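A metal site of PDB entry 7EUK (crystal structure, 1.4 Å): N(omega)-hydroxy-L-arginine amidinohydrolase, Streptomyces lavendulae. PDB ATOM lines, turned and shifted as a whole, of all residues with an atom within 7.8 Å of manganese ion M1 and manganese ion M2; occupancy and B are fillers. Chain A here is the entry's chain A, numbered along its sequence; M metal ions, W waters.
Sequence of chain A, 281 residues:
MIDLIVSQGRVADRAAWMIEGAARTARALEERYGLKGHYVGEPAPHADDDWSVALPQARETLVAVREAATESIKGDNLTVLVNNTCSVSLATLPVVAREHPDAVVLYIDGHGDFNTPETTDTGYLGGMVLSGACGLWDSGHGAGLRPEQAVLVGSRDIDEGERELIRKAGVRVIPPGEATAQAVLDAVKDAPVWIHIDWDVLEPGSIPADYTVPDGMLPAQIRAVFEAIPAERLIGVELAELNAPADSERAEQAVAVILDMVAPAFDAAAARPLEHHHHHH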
ATOM      1  N   THR A  85      14.373 -13.683 -29.008  1.00  0.00           N
ATOM      2  CA  THR A  85      15.764 -13.336 -29.311  1.00  0.00           C
ATOM      3  C   THR A  85      16.542 -13.109 -28.023  1.00  0.00           C
ATOM      4  O   THR A  85      15.958 -12.843 -26.963  1.00  0.00           O
ATOM      5  CB  THR A  85      15.872 -12.068 -30.162  1.00  0.00           C
ATOM      6  OG1 THR A  85      15.310 -10.968 -29.436  1.00  0.00           O
ATOM      7  CG2 THR A  85      15.147 -12.215 -31.497  1.00  0.00           C
ATOM      8  N   CYS A  86      17.865 -13.229 -28.120  1.00  0.00           N
ATOM      9  CA  CYS A  86      18.708 -12.890 -26.983  1.00  0.00           C
ATOM     10  C   CYS A  86      18.503 -11.462 -26.536  1.00  0.00           C
ATOM     11  O   CYS A  86      18.716 -11.167 -25.354  1.00  0.00           O
ATOM     12  CB  CYS A  86      20.178 -13.121 -27.312  1.00  0.00           C
ATOM     13  SG  CYS A  86      20.672 -14.853 -27.406  1.00  0.00           S
ATOM     14  N   SER A  87      18.103 -10.574 -27.459  1.00  0.00           N
ATOM     15  CA  SER A  87      17.984  -9.154 -27.115  1.00  0.00           C
ATOM     16  C   SER A  87      16.925  -8.875 -26.062  1.00  0.00           C
ATOM     17  O   SER A  87      16.991  -7.819 -25.407  1.00  0.00           O
ATOM     18  CB  SER A  87      17.670  -8.319 -28.358  1.00  0.00           C
ATOM     19  OG  SER A  87      18.729  -8.391 -29.288  1.00  0.00           O
ATOM     20  N   TYR A 107      26.113 -17.317 -19.866  1.00  0.00           N
ATOM     21  CA  TYR A 107      25.592 -16.862 -21.156  1.00  0.00           C
ATOM     22  C   TYR A 107      26.037 -17.904 -22.171  1.00  0.00           C
ATOM     23  O   TYR A 107      27.188 -17.899 -22.639  1.00  0.00           O
ATOM     24  CB  TYR A 107      26.102 -15.459 -21.453  1.00  0.00           C
ATOM     25  CG  TYR A 107      25.292 -14.707 -22.498  1.00  0.00           C
ATOM     26  CD1 TYR A 107      25.490 -14.955 -23.856  1.00  0.00           C
ATOM     27  CD2 TYR A 107      24.347 -13.751 -22.149  1.00  0.00           C
ATOM     28  CE1 TYR A 107      24.760 -14.286 -24.821  1.00  0.00           C
ATOM     29  CE2 TYR A 107      23.622 -13.063 -23.102  1.00  0.00           C
ATOM     30  CZ  TYR A 107      23.837 -13.341 -24.446  1.00  0.00           C
ATOM     31  OH  TYR A 107      23.117 -12.663 -25.418  1.00  0.00           O
ATOM     32  N   ILE A 108      25.147 -18.838 -22.455  1.00  0.00           N
ATOM     33  CA  ILE A 108      25.448 -20.035 -23.231  1.00  0.00           C
ATOM     34  C   ILE A 108      25.053 -19.743 -24.676  1.00  0.00           C
ATOM     35  O   ILE A 108      23.876 -19.631 -24.997  1.00  0.00           O
ATOM     36  CB  ILE A 108      24.726 -21.264 -22.661  1.00  0.00           C
ATOM     37  CG1 ILE A 108      24.990 -21.381 -21.149  1.00  0.00           C
ATOM     38  CG2 ILE A 108      25.172 -22.535 -23.407  1.00  0.00           C
ATOM     39  CD1 ILE A 108      24.382 -22.627 -20.519  1.00  0.00           C
ATOM     40  N   ASP A 109      26.039 -19.618 -25.556  1.00  0.00           N
ATOM     41  CA  ASP A 109      25.807 -19.034 -26.876  1.00  0.00           C
ATOM     42  C   ASP A 109      26.990 -19.397 -27.757  1.00  0.00           C
ATOM     43  O   ASP A 109      28.132 -19.402 -27.282  1.00  0.00           O
ATOM     44  CB  ASP A 109      25.698 -17.487 -26.714  1.00  0.00           C
ATOM     45  CG  ASP A 109      25.026 -16.808 -27.888  1.00  0.00           C
ATOM     46  OD1 ASP A 109      25.313 -17.169 -29.054  1.00  0.00           O
ATOM     47  OD2 ASP A 109      24.188 -15.894 -27.656  1.00  0.00           O
ATOM     48  N   GLY A 110      26.740 -19.713 -29.035  1.00  0.00           N
ATOM     49  CA  GLY A 110      27.856 -19.913 -29.940  1.00  0.00           C
ATOM     50  C   GLY A 110      28.613 -18.636 -30.246  1.00  0.00           C
ATOM     51  O   GLY A 110      29.757 -18.699 -30.749  1.00  0.00           O
ATOM     52  N   HIS A 111      28.003 -17.484 -29.959  1.00  0.00           N
ATOM     53  CA  HIS A 111      28.592 -16.167 -30.155  1.00  0.00           C
ATOM     54  C   HIS A 111      28.910 -15.532 -28.818  1.00  0.00           C
ATOM     55  O   HIS A 111      28.444 -15.978 -27.760  1.00  0.00           O
ATOM     56  CB  HIS A 111      27.593 -15.237 -30.853  1.00  0.00           C
ATOM     57  CG  HIS A 111      27.157 -15.720 -32.190  1.00  0.00           C
ATOM     58  ND1 HIS A 111      26.053 -16.530 -32.362  1.00  0.00           N
ATOM     59  CD2 HIS A 111      27.659 -15.512 -33.434  1.00  0.00           C
ATOM     60  CE1 HIS A 111      25.892 -16.793 -33.650  1.00  0.00           C
ATOM     61  NE2 HIS A 111      26.850 -16.184 -34.319  1.00  0.00           N
ATOM     62  N   GLY A 112      29.689 -14.441 -28.865  1.00  0.00           N
ATOM     63  CA  GLY A 112      29.949 -13.680 -27.653  1.00  0.00           C
ATOM     64  C   GLY A 112      28.878 -12.655 -27.302  1.00  0.00           C
ATOM     65  O   GLY A 112      28.762 -12.269 -26.139  1.00  0.00           O
ATOM     66  N   ASP A 113      28.101 -12.199 -28.301  1.00  0.00           N
ATOM     67  CA  ASP A 113      27.083 -11.164 -28.109  1.00  0.00           C
ATOM     68  C   ASP A 113      27.632  -9.978 -27.321  1.00  0.00           C
ATOM     69  O   ASP A 113      26.946  -9.412 -26.467  1.00  0.00           O
ATOM     70  CB  ASP A 113      25.813 -11.737 -27.464  1.00  0.00           C
ATOM     71  CG  ASP A 113      25.052 -12.664 -28.388  1.00  0.00           C
ATOM     72  OD1 ASP A 113      25.522 -12.945 -29.518  1.00  0.00           O
ATOM     73  OD2 ASP A 113      23.950 -13.092 -27.992  1.00  0.00           O
ATOM     74  N   TYR A 124      23.432  -5.511 -35.720  1.00  0.00           N
ATOM     75  CA  TYR A 124      22.381  -6.341 -35.148  1.00  0.00           C
ATOM     76  C   TYR A 124      22.384  -6.259 -33.611  1.00  0.00           C
ATOM     77  O   TYR A 124      23.389  -6.562 -32.962  1.00  0.00           O
ATOM     78  CB  TYR A 124      22.541  -7.787 -35.627  1.00  0.00           C
ATOM     79  CG  TYR A 124      21.549  -8.753 -35.035  1.00  0.00           C
ATOM     80  CD1 TYR A 124      20.194  -8.445 -34.961  1.00  0.00           C
ATOM     81  CD2 TYR A 124      21.982  -9.969 -34.545  1.00  0.00           C
ATOM     82  CE1 TYR A 124      19.292  -9.348 -34.409  1.00  0.00           C
ATOM     83  CE2 TYR A 124      21.097 -10.864 -33.978  1.00  0.00           C
ATOM     84  CZ  TYR A 124      19.745 -10.563 -33.909  1.00  0.00           C
ATOM     85  OH  TYR A 124      18.887 -11.480 -33.336  1.00  0.00           O
ATOM     86  N   GLY A 126      21.071  -8.165 -31.479  1.00  0.00           N
ATOM     87  CA  GLY A 126      21.292  -9.451 -30.842  1.00  0.00           C
ATOM     88  C   GLY A 126      22.757  -9.787 -30.653  1.00  0.00           C
ATOM     89  O   GLY A 126      23.075 -10.676 -29.856  1.00  0.00           O
ATOM     90  N   GLY A 127      23.657  -9.112 -31.354  1.00  0.00           N
ATOM     91  CA  GLY A 127      25.080  -9.282 -31.129  1.00  0.00           C
ATOM     92  C   GLY A 127      25.660  -8.344 -30.101  1.00  0.00           C
ATOM     93  O   GLY A 127      26.883  -8.314 -29.944  1.00  0.00           O
ATOM     94  N   MET A 128      24.809  -7.603 -29.386  1.00  0.00           N
ATOM     95  CA  MET A 128      25.227  -6.544 -28.476  1.00  0.00           C
ATOM     96  C   MET A 128      24.628  -6.716 -27.084  1.00  0.00           C
ATOM     97  O   MET A 128      24.665  -5.784 -26.279  1.00  0.00           O
ATOM     98  CB  MET A 128      24.796  -5.169 -29.038  1.00  0.00           C
ATOM     99  CG  MET A 128      25.290  -4.882 -30.458  1.00  0.00           C
ATOM    100  SD  MET A 128      24.446  -3.566 -31.369  1.00  0.00           S
ATOM    101  CE  MET A 128      24.888  -2.152 -30.382  1.00  0.00           C
ATOM    102  N   VAL A 129      24.084  -7.898 -26.786  1.00  0.00           N
ATOM    103  CA  VAL A 129      23.266  -8.084 -25.587  1.00  0.00           C
ATOM    104  C   VAL A 129      24.108  -8.097 -24.330  1.00  0.00           C
ATOM    105  O   VAL A 129      23.818  -7.384 -23.357  1.00  0.00           O
ATOM    106  CB  VAL A 129      22.435  -9.370 -25.722  1.00  0.00           C
ATOM    107  CG1 VAL A 129      21.619  -9.618 -24.456  1.00  0.00           C
ATOM    108  CG2 VAL A 129      21.532  -9.307 -26.936  1.00  0.00           C
ATOM    109  N   LEU A 130      25.132  -8.947 -24.280  1.00  0.00           N
ATOM    110  CA  LEU A 130      25.880  -9.094 -23.045  1.00  0.00           C
ATOM    111  C   LEU A 130      26.684  -7.839 -22.744  1.00  0.00           C
ATOM    112  O   LEU A 130      26.776  -7.411 -21.589  1.00  0.00           O
ATOM    113  CB  LEU A 130      26.750 -10.347 -23.090  1.00  0.00           C
ATOM    114  CG  LEU A 130      27.560 -10.705 -21.840  1.00  0.00           C
ATOM    115  CD1 LEU A 130      26.674 -10.915 -20.626  1.00  0.00           C
ATOM    116  CD2 LEU A 130      28.382 -11.938 -22.125  1.00  0.00           C
ATOM    117  N   SER A 155      30.958 -20.484 -26.603  1.00  0.00           N
ATOM    118  CA  SER A 155      31.272 -19.527 -27.650  1.00  0.00           C
ATOM    119  C   SER A 155      32.557 -19.935 -28.353  1.00  0.00           C
ATOM    120  O   SER A 155      33.478 -20.471 -27.748  1.00  0.00           O
ATOM    121  CB  SER A 155      31.475 -18.153 -27.020  1.00  0.00           C
ATOM    122  OG  SER A 155      30.409 -17.826 -26.154  1.00  0.00           O
ATOM    123  N   HIS A 196      21.296 -18.246 -19.366  1.00  0.00           N
ATOM    124  CA  HIS A 196      20.756 -17.706 -20.605  1.00  0.00           C
ATOM    125  C   HIS A 196      21.274 -18.571 -21.750  1.00  0.00           C
ATOM    126  O   HIS A 196      22.486 -18.719 -21.915  1.00  0.00           O
ATOM    127  CB  HIS A 196      21.265 -16.272 -20.770  1.00  0.00           C
ATOM    128  CG  HIS A 196      20.998 -15.666 -22.119  1.00  0.00           C
ATOM    129  ND1 HIS A 196      20.091 -14.641 -22.293  1.00  0.00           N
ATOM    130  CD2 HIS A 196      21.515 -15.941 -23.338  1.00  0.00           C
ATOM    131  CE1 HIS A 196      20.056 -14.309 -23.581  1.00  0.00           C
ATOM    132  NE2 HIS A 196      20.905 -15.093 -24.240  1.00  0.00           N
ATOM    133  N   ILE A 197      20.368 -19.151 -22.546  1.00  0.00           N
ATOM    134  CA  ILE A 197      20.772 -20.028 -23.661  1.00  0.00           C
ATOM    135  C   ILE A 197      20.289 -19.473 -24.995  1.00  0.00           C
ATOM    136  O   ILE A 197      19.098 -19.189 -25.155  1.00  0.00           O
ATOM    137  CB  ILE A 197      20.273 -21.465 -23.487  1.00  0.00           C
ATOM    138  CG1 ILE A 197      20.858 -22.088 -22.237  1.00  0.00           C
ATOM    139  CG2 ILE A 197      20.676 -22.307 -24.700  1.00  0.00           C
ATOM    140  CD1 ILE A 197      20.152 -23.388 -21.843  1.00  0.00           C
ATOM    141  N   ASP A 198      21.219 -19.348 -25.955  1.00  0.00           N
ATOM    142  CA  ASP A 198      20.936 -19.162 -27.378  1.00  0.00           C
ATOM    143  C   ASP A 198      21.200 -20.513 -28.036  1.00  0.00           C
ATOM    144  O   ASP A 198      22.322 -21.023 -27.992  1.00  0.00           O
ATOM    145  CB  ASP A 198      21.899 -18.091 -27.880  1.00  0.00           C
ATOM    146  CG  ASP A 198      21.841 -17.820 -29.393  1.00  0.00           C
ATOM    147  OD1 ASP A 198      21.283 -18.642 -30.132  1.00  0.00           O
ATOM    148  OD2 ASP A 198      22.427 -16.775 -29.819  1.00  0.00           O
ATOM    149  N   TRP A 199      20.161 -21.092 -28.655  1.00  0.00           N
ATOM    150  CA  TRP A 199      20.301 -22.450 -29.192  1.00  0.00           C
ATOM    151  C   TRP A 199      21.341 -22.580 -30.297  1.00  0.00           C
ATOM    152  O   TRP A 199      21.709 -23.723 -30.610  1.00  0.00           O
ATOM    153  CB  TRP A 199      18.946 -23.034 -29.665  1.00  0.00           C
ATOM    154  CG  TRP A 199      17.958 -23.118 -28.546  1.00  0.00           C
ATOM    155  CD1 TRP A 199      16.746 -22.479 -28.477  1.00  0.00           C
ATOM    156  CD2 TRP A 199      18.085 -23.877 -27.339  1.00  0.00           C
ATOM    157  NE1 TRP A 199      16.122 -22.785 -27.301  1.00  0.00           N
ATOM    158  CE2 TRP A 199      16.928 -23.638 -26.574  1.00  0.00           C
ATOM    159  CE3 TRP A 199      19.074 -24.721 -26.812  1.00  0.00           C
ATOM    160  CZ2 TRP A 199      16.715 -24.218 -25.320  1.00  0.00           C
ATOM    161  CZ3 TRP A 199      18.866 -25.284 -25.560  1.00  0.00           C
ATOM    162  CH2 TRP A 199      17.699 -25.033 -24.834  1.00  0.00           C
ATOM    163  N   ASP A 200      21.827 -21.471 -30.874  1.00  0.00           N
ATOM    164  CA  ASP A 200      22.915 -21.629 -31.832  1.00  0.00           C
ATOM    165  C   ASP A 200      24.220 -22.126 -31.196  1.00  0.00           C
ATOM    166  O   ASP A 200      25.179 -22.420 -31.915  1.00  0.00           O
ATOM    167  CB  ASP A 200      23.121 -20.394 -32.730  1.00  0.00           C
ATOM    168  CG  ASP A 200      23.633 -19.180 -31.979  1.00  0.00           C
ATOM    169  OD1 ASP A 200      24.341 -19.301 -30.955  1.00  0.00           O
ATOM    170  OD2 ASP A 200      23.348 -18.045 -32.446  1.00  0.00           O
ATOM    171  N   VAL A 201      24.259 -22.278 -29.867  1.00  0.00           N
ATOM    172  CA  VAL A 201      25.420 -22.917 -29.253  1.00  0.00           C
ATOM    173  C   VAL A 201      25.526 -24.385 -29.642  1.00  0.00           C
ATOM    174  O   VAL A 201      26.636 -24.953 -29.613  1.00  0.00           O
ATOM    175  CB  VAL A 201      25.344 -22.745 -27.717  1.00  0.00           C
ATOM    176  CG1 VAL A 201      24.310 -23.681 -27.099  1.00  0.00           C
ATOM    177  CG2 VAL A 201      26.724 -22.962 -27.088  1.00  0.00           C
ATOM    178  N   ALA A 240      16.320 -19.004 -25.626  1.00  0.00           N
ATOM    179  CA  ALA A 240      16.194 -18.036 -26.711  1.00  0.00           C
ATOM    180  C   ALA A 240      16.649 -18.590 -28.058  1.00  0.00           C
ATOM    181  O   ALA A 240      17.530 -19.449 -28.133  1.00  0.00           O
ATOM    182  CB  ALA A 240      17.004 -16.771 -26.403  1.00  0.00           C
ATOM    183  N   GLU A 241      16.016 -18.074 -29.119  1.00  0.00           N
ATOM    184  CA  GLU A 241      16.491 -18.226 -30.504  1.00  0.00           C
ATOM    185  C   GLU A 241      16.325 -19.649 -31.050  1.00  0.00           C
ATOM    186  O   GLU A 241      17.239 -20.206 -31.667  1.00  0.00           O
ATOM    187  CB  GLU A 241      17.901 -17.662 -30.704  1.00  0.00           C
ATOM    188  CG  GLU A 241      18.044 -16.282 -30.112  1.00  0.00           C
ATOM    189  CD  GLU A 241      18.903 -15.331 -30.920  1.00  0.00           C
ATOM    190  OE1 GLU A 241      19.559 -15.757 -31.905  1.00  0.00           O
ATOM    191  OE2 GLU A 241      18.972 -14.135 -30.535  1.00  0.00           O
HETATM  192 MN    MN M   1      22.740 -14.801 -28.788  1.00  0.00          MN
HETATM  193 MN    MN M   2      24.357 -16.910 -30.899  1.00  0.00          MN
HETATM  194  O   HOH W   1      24.093 -14.706 -30.732  1.00  0.00           O
HETATM  195  O   HOH W   2      21.681 -13.494 -30.172  1.00  0.00           O
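Water W2 bridges the side-chain carboxylate of Glu 241 (2.8 Å) and the backbone carbonyl oxygen of Gly 126 (3.2 Å).
O of Asp 113 sits at hydrogen-bond distance from N of Val 129. O of His 111 lies within hydrogen-bond range of OG of Ser 155 (3.1 Å). SG of Cys 86 lies close to NE2 of His 196, at 3.2 Å. OE2 of Glu 241 is in hydrogen-bond range of N of Cys 86 (2.8 Å). O of Asp 113 lies within hydrogen-bond range of N of Leu 130. The side-chain carboxylate of Asp 200 sits close to the backbone NH of Gly 110 (3.1 Å). The backbone NH (N) of Asp 198 sits at hydrogen-bond distance from the backbone carbonyl oxygen (O) of Ile 108. OH of Tyr 107 lies close to OD2 of Asp 113.
Manganese ion M1 is bound by OD2 of Asp 109 (2.1 Å), water W2 (2.2 Å), OD2 of Asp 113 (2.2 Å), OD2 of Asp 198 (2.2 Å), water W1 (2.4 Å) and SG of Cys 86 (2.5 Å).
Manganese ion M2 is bound by the side-chain carboxylate (OD1) of Asp 109. Manganese ion M2 is bound by OD2 of Asp 200, 2.2 Å away. OD2 of Asp 198 binds manganese ion M2, at 2.2 Å. Manganese ion M2 is bound by water W1 (2.2 Å). Manganese ion M2 is bound by a ring nitrogen (ND1) of His 111, 2.3 Å away. Manganese ion M2 is bound by the side-chain carboxylate (OD1) of Asp 200.
Four residues have an atom within 4 Å of manganese ion M2: Asp 109, His 111, Asp 198 and Asp 200. Along chain A the residues within 4 Å of manganese ion M2 span positions 109 to 200.
Of the 25 residues printed, 4 come within 4 Å of manganese ion M1. The nearest printed residue that does not touch manganese ion M1 is Tyr 107 (4.01 Å).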
